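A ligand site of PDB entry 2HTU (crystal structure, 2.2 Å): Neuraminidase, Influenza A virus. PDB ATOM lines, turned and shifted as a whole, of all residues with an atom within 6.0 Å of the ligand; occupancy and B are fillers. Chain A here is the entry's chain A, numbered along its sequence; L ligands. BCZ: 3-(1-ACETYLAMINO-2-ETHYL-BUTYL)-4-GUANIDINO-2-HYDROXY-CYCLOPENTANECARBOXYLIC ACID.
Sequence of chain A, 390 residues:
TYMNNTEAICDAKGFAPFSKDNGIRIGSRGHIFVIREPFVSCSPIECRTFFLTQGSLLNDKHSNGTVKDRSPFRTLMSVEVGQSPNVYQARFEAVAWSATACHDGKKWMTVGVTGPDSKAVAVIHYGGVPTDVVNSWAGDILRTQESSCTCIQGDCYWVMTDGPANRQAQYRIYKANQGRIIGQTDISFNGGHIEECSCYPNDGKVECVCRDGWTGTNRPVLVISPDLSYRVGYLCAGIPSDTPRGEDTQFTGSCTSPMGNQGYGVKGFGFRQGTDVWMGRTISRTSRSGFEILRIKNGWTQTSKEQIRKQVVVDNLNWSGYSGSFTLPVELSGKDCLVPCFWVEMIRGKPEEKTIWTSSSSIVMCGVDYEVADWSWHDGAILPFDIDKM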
ATOM      1  N   ARG A  36     -13.960  26.522  28.837  1.00  0.00           N
ATOM      2  CA  ARG A  36     -13.803  27.417  27.702  1.00  0.00           C
ATOM      3  C   ARG A  36     -14.906  28.469  27.886  1.00  0.00           C
ATOM      4  O   ARG A  36     -15.849  28.236  28.650  1.00  0.00           O
ATOM      5  CB  ARG A  36     -13.954  26.611  26.403  1.00  0.00           C
ATOM      6  CG  ARG A  36     -13.505  27.327  25.141  1.00  0.00           C
ATOM      7  CD  ARG A  36     -12.053  27.804  25.136  1.00  0.00           C
ATOM      8  NE  ARG A  36     -12.017  29.154  24.565  1.00  0.00           N
ATOM      9  CZ  ARG A  36     -12.359  29.470  23.321  1.00  0.00           C
ATOM     10  NH1 ARG A  36     -12.298  30.735  22.911  1.00  0.00           N
ATOM     11  NH2 ARG A  36     -12.749  28.535  22.462  1.00  0.00           N
ATOM     12  N   GLU A  37     -14.767  29.617  27.229  1.00  0.00           N
ATOM     13  CA  GLU A  37     -15.745  30.714  27.326  1.00  0.00           C
ATOM     14  C   GLU A  37     -16.138  31.163  28.730  1.00  0.00           C
ATOM     15  O   GLU A  37     -17.297  31.052  29.112  1.00  0.00           O
ATOM     16  CB  GLU A  37     -17.049  30.393  26.575  1.00  0.00           C
ATOM     17  CG  GLU A  37     -16.906  30.082  25.101  1.00  0.00           C
ATOM     18  CD  GLU A  37     -16.253  28.744  24.864  1.00  0.00           C
ATOM     19  OE1 GLU A  37     -16.486  27.820  25.670  1.00  0.00           O
ATOM     20  OE2 GLU A  37     -15.511  28.616  23.880  1.00  0.00           O
ATOM     21  N   LEU A  52     -18.130  27.373  30.694  1.00  0.00           N
ATOM     22  CA  LEU A  52     -18.669  26.221  30.000  1.00  0.00           C
ATOM     23  C   LEU A  52     -17.735  25.029  30.218  1.00  0.00           C
ATOM     24  O   LEU A  52     -16.617  24.986  29.697  1.00  0.00           O
ATOM     25  CB  LEU A  52     -18.811  26.520  28.512  1.00  0.00           C
ATOM     26  CG  LEU A  52     -19.741  27.698  28.168  1.00  0.00           C
ATOM     27  CD1 LEU A  52     -19.848  27.836  26.662  1.00  0.00           C
ATOM     28  CD2 LEU A  52     -21.116  27.455  28.773  1.00  0.00           C
ATOM     29  N   LYS A  68     -13.743  20.643  20.506  1.00  0.00           N
ATOM     30  CA  LYS A  68     -14.933  20.523  19.657  1.00  0.00           C
ATOM     31  C   LYS A  68     -16.092  21.527  19.817  1.00  0.00           C
ATOM     32  O   LYS A  68     -17.135  21.368  19.168  1.00  0.00           O
ATOM     33  CB  LYS A  68     -15.475  19.101  19.772  1.00  0.00           C
ATOM     34  CG  LYS A  68     -15.646  18.605  21.202  1.00  0.00           C
ATOM     35  CD  LYS A  68     -15.907  17.106  21.239  1.00  0.00           C
ATOM     36  CE  LYS A  68     -16.088  16.601  22.666  1.00  0.00           C
ATOM     37  NZ  LYS A  68     -16.392  15.142  22.665  1.00  0.00           N
ATOM     38  N   ASP A  69     -15.912  22.546  20.662  1.00  0.00           N
ATOM     39  CA  ASP A  69     -16.949  23.561  20.868  1.00  0.00           C
ATOM     40  C   ASP A  69     -18.304  23.094  21.402  1.00  0.00           C
ATOM     41  O   ASP A  69     -18.802  23.660  22.370  1.00  0.00           O
ATOM     42  CB  ASP A  69     -17.185  24.368  19.587  1.00  0.00           C
ATOM     43  CG  ASP A  69     -16.083  25.375  19.294  1.00  0.00           C
ATOM     44  OD1 ASP A  69     -15.549  25.975  20.253  1.00  0.00           O
ATOM     45  OD2 ASP A  69     -15.759  25.584  18.111  1.00  0.00           O
ATOM     46  N   ARG A  70     -18.893  22.076  20.793  1.00  0.00           N
ATOM     47  CA  ARG A  70     -20.209  21.602  21.224  1.00  0.00           C
ATOM     48  C   ARG A  70     -20.333  20.096  21.440  1.00  0.00           C
ATOM     49  O   ARG A  70     -19.841  19.297  20.660  1.00  0.00           O
ATOM     50  CB  ARG A  70     -21.281  22.076  20.221  1.00  0.00           C
ATOM     51  CG  ARG A  70     -21.269  23.581  19.987  1.00  0.00           C
ATOM     52  CD  ARG A  70     -22.330  24.029  18.993  1.00  0.00           C
ATOM     53  NE  ARG A  70     -22.195  23.369  17.707  1.00  0.00           N
ATOM     54  CZ  ARG A  70     -21.173  23.511  16.867  1.00  0.00           C
ATOM     55  NH1 ARG A  70     -21.155  22.840  15.731  1.00  0.00           N
ATOM     56  NH2 ARG A  70     -20.168  24.345  17.157  1.00  0.00           N
ATOM     57  N   ARG A  74     -21.407  19.294  27.686  1.00  0.00           N
ATOM     58  CA  ARG A  74     -21.092  20.681  27.983  1.00  0.00           C
ATOM     59  C   ARG A  74     -22.127  21.293  28.933  1.00  0.00           C
ATOM     60  O   ARG A  74     -23.325  21.245  28.640  1.00  0.00           O
ATOM     61  CB  ARG A  74     -21.047  21.479  26.673  1.00  0.00           C
ATOM     62  CG  ARG A  74     -20.029  22.610  26.631  1.00  0.00           C
ATOM     63  CD  ARG A  74     -18.680  22.101  26.158  1.00  0.00           C
ATOM     64  NE  ARG A  74     -17.594  23.037  26.456  1.00  0.00           N
ATOM     65  CZ  ARG A  74     -17.389  24.182  25.814  1.00  0.00           C
ATOM     66  NH1 ARG A  74     -16.386  24.969  26.153  1.00  0.00           N
ATOM     67  NH2 ARG A  74     -18.189  24.539  24.809  1.00  0.00           N
ATOM     68  N   TRP A  97     -23.604  24.558  25.648  1.00  0.00           N
ATOM     69  CA  TRP A  97     -22.329  24.691  24.964  1.00  0.00           C
ATOM     70  C   TRP A  97     -22.223  26.154  24.494  1.00  0.00           C
ATOM     71  O   TRP A  97     -21.307  26.515  23.763  1.00  0.00           O
ATOM     72  CB  TRP A  97     -22.179  23.703  23.794  1.00  0.00           C
ATOM     73  CG  TRP A  97     -23.426  23.292  23.057  1.00  0.00           C
ATOM     74  CD1 TRP A  97     -24.028  22.063  23.090  1.00  0.00           C
ATOM     75  CD2 TRP A  97     -24.195  24.093  22.143  1.00  0.00           C
ATOM     76  NE1 TRP A  97     -25.112  22.041  22.245  1.00  0.00           N
ATOM     77  CE2 TRP A  97     -25.239  23.275  21.652  1.00  0.00           C
ATOM     78  CE3 TRP A  97     -24.098  25.412  21.684  1.00  0.00           C
ATOM     79  CZ2 TRP A  97     -26.187  23.726  20.726  1.00  0.00           C
ATOM     80  CZ3 TRP A  97     -25.041  25.864  20.765  1.00  0.00           C
ATOM     81  CH2 TRP A  97     -26.075  25.027  20.296  1.00  0.00           C
ATOM     82  N   SER A  98     -23.174  26.965  24.954  1.00  0.00           N
ATOM     83  CA  SER A  98     -23.248  28.387  24.674  1.00  0.00           C
ATOM     84  C   SER A  98     -24.135  28.958  25.801  1.00  0.00           C
ATOM     85  O   SER A  98     -25.137  28.356  26.166  1.00  0.00           O
ATOM     86  CB  SER A  98     -23.869  28.665  23.303  1.00  0.00           C
ATOM     87  OG  SER A  98     -24.015  30.070  23.055  1.00  0.00           O
ATOM     88  N   ALA A  99     -23.779  30.125  26.350  1.00  0.00           N
ATOM     89  CA  ALA A  99     -24.558  30.679  27.464  1.00  0.00           C
ATOM     90  C   ALA A  99     -24.415  32.162  27.717  1.00  0.00           C
ATOM     91  O   ALA A  99     -23.642  32.849  27.088  1.00  0.00           O
ATOM     92  CB  ALA A  99     -24.209  29.935  28.738  1.00  0.00           C
ATOM     93  N   ILE A 141     -27.166  26.250  14.749  1.00  0.00           N
ATOM     94  CA  ILE A 141     -26.422  26.601  15.942  1.00  0.00           C
ATOM     95  C   ILE A 141     -26.963  27.855  16.653  1.00  0.00           C
ATOM     96  O   ILE A 141     -26.342  28.915  16.616  1.00  0.00           O
ATOM     97  CB  ILE A 141     -24.916  26.823  15.635  1.00  0.00           C
ATOM     98  CG1 ILE A 141     -24.386  25.665  14.774  1.00  0.00           C
ATOM     99  CG2 ILE A 141     -24.118  26.887  16.921  1.00  0.00           C
ATOM    100  CD1 ILE A 141     -22.916  25.784  14.439  1.00  0.00           C
ATOM    101  N   LEU A 142     -28.142  27.736  17.278  1.00  0.00           N
ATOM    102  CA  LEU A 142     -28.706  28.865  18.019  1.00  0.00           C
ATOM    103  C   LEU A 142     -27.680  29.131  19.123  1.00  0.00           C
ATOM    104  O   LEU A 142     -27.334  28.207  19.870  1.00  0.00           O
ATOM    105  CB  LEU A 142     -30.063  28.489  18.637  1.00  0.00           C
ATOM    106  CG  LEU A 142     -30.527  29.392  19.802  1.00  0.00           C
ATOM    107  CD1 LEU A 142     -30.931  30.744  19.251  1.00  0.00           C
ATOM    108  CD2 LEU A 142     -31.702  28.741  20.541  1.00  0.00           C
ATOM    109  N   ARG A 143     -27.197  30.363  19.239  1.00  0.00           N
ATOM    110  CA  ARG A 143     -26.168  30.687  20.228  1.00  0.00           C
ATOM    111  C   ARG A 143     -26.291  32.081  20.832  1.00  0.00           C
ATOM    112  O   ARG A 143     -27.076  32.916  20.362  1.00  0.00           O
ATOM    113  CB  ARG A 143     -24.780  30.527  19.595  1.00  0.00           C
ATOM    114  CG  ARG A 143     -24.589  31.294  18.285  1.00  0.00           C
ATOM    115  CD  ARG A 143     -23.365  30.770  17.504  1.00  0.00           C
ATOM    116  NE  ARG A 143     -23.153  31.502  16.261  1.00  0.00           N
ATOM    117  CZ  ARG A 143     -23.823  31.277  15.127  1.00  0.00           C
ATOM    118  NH1 ARG A 143     -23.560  32.014  14.047  1.00  0.00           N
ATOM    119  NH2 ARG A 143     -24.742  30.330  15.073  1.00  0.00           N
ATOM    120  N   GLU A 146     -21.865  34.591  25.539  1.00  0.00           N
ATOM    121  CA  GLU A 146     -20.651  34.035  26.116  1.00  0.00           C
ATOM    122  C   GLU A 146     -20.089  35.071  27.068  1.00  0.00           C
ATOM    123  O   GLU A 146     -18.908  35.027  27.429  1.00  0.00           O
ATOM    124  CB  GLU A 146     -19.601  33.684  25.053  1.00  0.00           C
ATOM    125  CG  GLU A 146     -20.137  32.834  23.919  1.00  0.00           C
ATOM    126  CD  GLU A 146     -20.726  31.505  24.352  1.00  0.00           C
ATOM    127  OE1 GLU A 146     -21.345  31.416  25.439  1.00  0.00           O
ATOM    128  OE2 GLU A 146     -20.588  30.528  23.592  1.00  0.00           O
ATOM    129  N   ALA A 165     -21.890  30.999  10.337  1.00  0.00           N
ATOM    130  CA  ALA A 165     -20.849  31.684  11.096  1.00  0.00           C
ATOM    131  C   ALA A 165     -19.900  32.447  10.160  1.00  0.00           C
ATOM    132  O   ALA A 165     -18.893  33.004  10.617  1.00  0.00           O
ATOM    133  CB  ALA A 165     -20.065  30.687  11.937  1.00  0.00           C
ATOM    134  N   GLU A 195     -22.001  38.325  16.456  1.00  0.00           N
ATOM    135  CA  GLU A 195     -21.713  37.150  17.271  1.00  0.00           C
ATOM    136  C   GLU A 195     -21.221  37.598  18.642  1.00  0.00           C
ATOM    137  O   GLU A 195     -20.685  38.697  18.783  1.00  0.00           O
ATOM    138  CB  GLU A 195     -20.565  36.323  16.669  1.00  0.00           C
ATOM    139  CG  GLU A 195     -20.822  35.682  15.327  1.00  0.00           C
ATOM    140  CD  GLU A 195     -21.504  34.329  15.444  1.00  0.00           C
ATOM    141  OE1 GLU A 195     -21.547  33.597  14.428  1.00  0.00           O
ATOM    142  OE2 GLU A 195     -22.009  33.995  16.534  1.00  0.00           O
ATOM    143  N   GLU A 196     -21.429  36.726  19.620  1.00  0.00           N
ATOM    144  CA  GLU A 196     -20.972  36.908  20.994  1.00  0.00           C
ATOM    145  C   GLU A 196     -20.883  38.347  21.484  1.00  0.00           C
ATOM    146  O   GLU A 196     -19.808  38.831  21.843  1.00  0.00           O
ATOM    147  CB  GLU A 196     -19.620  36.225  21.132  1.00  0.00           C
ATOM    148  CG  GLU A 196     -19.575  34.861  20.441  1.00  0.00           C
ATOM    149  CD  GLU A 196     -18.185  34.256  20.359  1.00  0.00           C
ATOM    150  OE1 GLU A 196     -17.255  34.945  19.879  1.00  0.00           O
ATOM    151  OE2 GLU A 196     -18.024  33.097  20.786  1.00  0.00           O
ATOM    152  N   ARG A 211     -18.923  40.733  17.676  1.00  0.00           N
ATOM    153  CA  ARG A 211     -17.942  40.107  16.780  1.00  0.00           C
ATOM    154  C   ARG A 211     -18.534  39.793  15.406  1.00  0.00           C
ATOM    155  O   ARG A 211     -19.604  39.190  15.305  1.00  0.00           O
ATOM    156  CB  ARG A 211     -17.406  38.822  17.434  1.00  0.00           C
ATOM    157  CG  ARG A 211     -16.651  37.845  16.523  1.00  0.00           C
ATOM    158  CD  ARG A 211     -16.286  36.558  17.291  1.00  0.00           C
ATOM    159  NE  ARG A 211     -15.765  35.485  16.432  1.00  0.00           N
ATOM    160  CZ  ARG A 211     -15.507  34.242  16.854  1.00  0.00           C
ATOM    161  NH1 ARG A 211     -15.032  33.335  16.009  1.00  0.00           N
ATOM    162  NH2 ARG A 211     -15.729  33.900  18.127  1.00  0.00           N
ATOM    163  N   TYR A 264     -12.566  35.357   9.830  1.00  0.00           N
ATOM    164  CA  TYR A 264     -12.742  34.840  11.180  1.00  0.00           C
ATOM    165  C   TYR A 264     -12.989  35.865  12.299  1.00  0.00           C
ATOM    166  O   TYR A 264     -13.744  36.812  12.124  1.00  0.00           O
ATOM    167  CB  TYR A 264     -11.553  33.955  11.539  1.00  0.00           C
ATOM    168  CG  TYR A 264     -11.866  32.894  12.558  1.00  0.00           C
ATOM    169  CD1 TYR A 264     -12.984  32.056  12.389  1.00  0.00           C
ATOM    170  CD2 TYR A 264     -11.055  32.691  13.674  1.00  0.00           C
ATOM    171  CE1 TYR A 264     -13.280  31.050  13.321  1.00  0.00           C
ATOM    172  CE2 TYR A 264     -11.346  31.686  14.614  1.00  0.00           C
ATOM    173  CZ  TYR A 264     -12.463  30.875  14.427  1.00  0.00           C
ATOM    174  OH  TYR A 264     -12.768  29.880  15.326  1.00  0.00           O
ATOM    175  N   GLY A 265     -12.375  35.657  13.461  1.00  0.00           N
ATOM    176  CA  GLY A 265     -12.555  36.598  14.548  1.00  0.00           C
ATOM    177  C   GLY A 265     -12.431  36.016  15.941  1.00  0.00           C
ATOM    178  O   GLY A 265     -12.099  34.842  16.120  1.00  0.00           O
ATOM    179  N   VAL A 266     -12.713  36.853  16.935  1.00  0.00           N
ATOM    180  CA  VAL A 266     -12.647  36.470  18.345  1.00  0.00           C
ATOM    181  C   VAL A 266     -13.543  37.401  19.156  1.00  0.00           C
ATOM    182  O   VAL A 266     -13.652  38.583  18.837  1.00  0.00           O
ATOM    183  CB  VAL A 266     -11.209  36.600  18.885  1.00  0.00           C
ATOM    184  CG1 VAL A 266     -10.706  38.034  18.733  1.00  0.00           C
ATOM    185  CG2 VAL A 266     -11.184  36.193  20.367  1.00  0.00           C
ATOM    186  N   ARG A 288      -4.205  34.620  18.679  1.00  0.00           N
ATOM    187  CA  ARG A 288      -4.832  34.939  19.954  1.00  0.00           C
ATOM    188  C   ARG A 288      -3.780  34.929  21.056  1.00  0.00           C
ATOM    189  O   ARG A 288      -3.742  34.043  21.920  1.00  0.00           O
ATOM    190  CB  ARG A 288      -5.945  33.931  20.255  1.00  0.00           C
ATOM    191  CG  ARG A 288      -7.108  34.060  19.286  1.00  0.00           C
ATOM    192  CD  ARG A 288      -8.209  33.045  19.567  1.00  0.00           C
ATOM    193  NE  ARG A 288      -9.362  33.306  18.715  1.00  0.00           N
ATOM    194  CZ  ARG A 288     -10.496  32.629  18.752  1.00  0.00           C
ATOM    195  NH1 ARG A 288     -11.484  32.958  17.929  1.00  0.00           N
ATOM    196  NH2 ARG A 288     -10.661  31.627  19.599  1.00  0.00           N
ATOM    197  N   TYR A 322     -10.808  34.965  24.229  1.00  0.00           N
ATOM    198  CA  TYR A 322     -12.018  35.744  24.483  1.00  0.00           C
ATOM    199  C   TYR A 322     -11.858  36.844  25.528  1.00  0.00           C
ATOM    200  O   TYR A 322     -10.887  36.869  26.294  1.00  0.00           O
ATOM    201  CB  TYR A 322     -13.151  34.797  24.887  1.00  0.00           C
ATOM    202  CG  TYR A 322     -13.872  34.156  23.710  1.00  0.00           C
ATOM    203  CD1 TYR A 322     -13.213  33.927  22.506  1.00  0.00           C
ATOM    204  CD2 TYR A 322     -15.199  33.752  23.822  1.00  0.00           C
ATOM    205  CE1 TYR A 322     -13.858  33.307  21.433  1.00  0.00           C
ATOM    206  CE2 TYR A 322     -15.850  33.132  22.765  1.00  0.00           C
ATOM    207  CZ  TYR A 322     -15.174  32.914  21.572  1.00  0.00           C
ATOM    208  OH  TYR A 322     -15.823  32.315  20.509  1.00  0.00           O
HETATM  209  C2  BCZ L   1     -17.154  28.629  20.222  1.00  0.00           C
HETATM  210  N25 BCZ L   1     -18.150  28.873  21.268  1.00  0.00           N
HETATM  211  C26 BCZ L   1     -18.503  27.936  22.090  1.00  0.00           C
HETATM  212  N30 BCZ L   1     -18.038  26.646  22.119  1.00  0.00           N
HETATM  213  N27 BCZ L   1     -19.431  28.244  23.048  1.00  0.00           N
HETATM  214  C3  BCZ L   1     -17.487  29.447  18.935  1.00  0.00           C
HETATM  215  C10 BCZ L   1     -18.723  29.013  18.043  1.00  0.00           C
HETATM  216  C24 BCZ L   1     -18.908  29.989  16.766  1.00  0.00           C
HETATM  217  C37 BCZ L   1     -19.136  31.482  17.201  1.00  0.00           C
HETATM  218  C38 BCZ L   1     -18.538  32.579  16.293  1.00  0.00           C
HETATM  219  C36 BCZ L   1     -20.125  29.487  15.887  1.00  0.00           C
HETATM  220  C39 BCZ L   1     -20.017  28.025  15.371  1.00  0.00           C
HETATM  221  N11 BCZ L   1     -19.957  29.033  18.843  1.00  0.00           N
HETATM  222  C13 BCZ L   1     -20.540  27.858  19.216  1.00  0.00           C
HETATM  223  C15 BCZ L   1     -21.809  27.916  20.046  1.00  0.00           C
HETATM  224  O14 BCZ L   1     -20.122  26.749  18.943  1.00  0.00           O
HETATM  225  C4  BCZ L   1     -16.140  29.420  18.141  1.00  0.00           C
HETATM  226  O9  BCZ L   1     -16.144  28.257  17.245  1.00  0.00           O
HETATM  227  C5  BCZ L   1     -15.001  29.235  19.189  1.00  0.00           C
HETATM  228  C6  BCZ L   1     -13.946  30.293  19.147  1.00  0.00           C
HETATM  229  O8  BCZ L   1     -13.058  30.394  19.982  1.00  0.00           O
HETATM  230  O7  BCZ L   1     -13.976  31.169  18.127  1.00  0.00           O
HETATM  231  C1  BCZ L   1     -15.722  29.147  20.564  1.00  0.00           C
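The guanidinium group of Arg 70 sits at hydrogen-bond distance from an oxygen (O14) of the ligand, 3.0 Å away.
O8 of the ligand lies within salt-bridge range of NH2 of Arg 288 (2.7 Å).
NH1 of Arg 36 lies within salt-bridge range of O8 of the ligand.
The backbone carbonyl oxygen of Asp 69 is in hydrogen-bond range of a nitrogen (N30) of the ligand, at 3.1 Å.
An oxygen (O7) of the ligand is in hydrogen-bond range of the side-chain hydroxyl (OH) of Tyr 264, 3.3 Å away.
A nitrogen (N27) of the ligand lies within salt-bridge range of the side-chain carboxylate (OE2) of Glu 146, 2.6 Å away.
OE2 of Glu 37 lies within salt-bridge range of N30 of the ligand, at 3.7 Å.
An oxygen (O7) of the ligand lies close to the side-chain hydroxyl of Tyr 322, at 3.2 Å.
NH1 of Arg 211 lies within salt-bridge range of O7 of the ligand (3.2 Å).
O of Trp 97 lies within hydrogen-bond range of N27 of the ligand, 2.6 Å away.
The side-chain carboxylate of Asp 69 lies within salt-bridge range of a nitrogen (N30) of the ligand.
The backbone carbonyl oxygen of Arg 36 lies within hydrogen-bond range of the backbone NH of Leu 52 (3.2 Å).
NH2 of Arg 143 sits at hydrogen-bond distance from O of Ile 141 (2.6 Å).
The guanidinium group (NH1) of Arg 143 is in salt-bridge range of the side-chain carboxylate (OE1) of Glu 195.
NH2 of Arg 74 is in hydrogen-bond range of O of Asp 69 (2.7 Å).
The guanidinium group (NH2) of Arg 36 is in salt-bridge range of the side-chain carboxylate (OE2) of Glu 37, 3.1 Å away.
The side-chain hydroxyl (OH) of Tyr 322 sits at hydrogen-bond distance from the side-chain carboxylate (OE1) of Glu 196, 3.1 Å away.
The side-chain carboxylate of Glu 146 sits at hydrogen-bond distance from the side-chain hydroxyl of Ser 98.
NH1 of Arg 211 lies within hydrogen-bond range of O of Gly 265.
The guanidinium group of Arg 74 lies close to a nitrogen (N30) of the ligand, at 3.4 Å.
Residues that only touch the ligand: Glu 195 (3.5 Å), Arg 143 (3.7 Å), Leu 52 (3.7 Å), Ile 141 (3.8 Å) and Ser 98 (3.9 Å).
Hydrophobic or aromatic side chains that line the ligand: Leu 52, Trp 97, Ile 141 and Tyr 322.
16 residues have an atom within 4 Å of the ligand: Arg 36, Glu 37, Leu 52, Asp 69, Arg 70, Arg 74, Trp 97, Ser 98, Ile 141, Arg 143, Glu 146, Glu 195, Arg 211, Tyr 264, Arg 288 and Tyr 322.
The nearest printed residue that does not touch the ligand is Glu 196 (4.1 Å).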
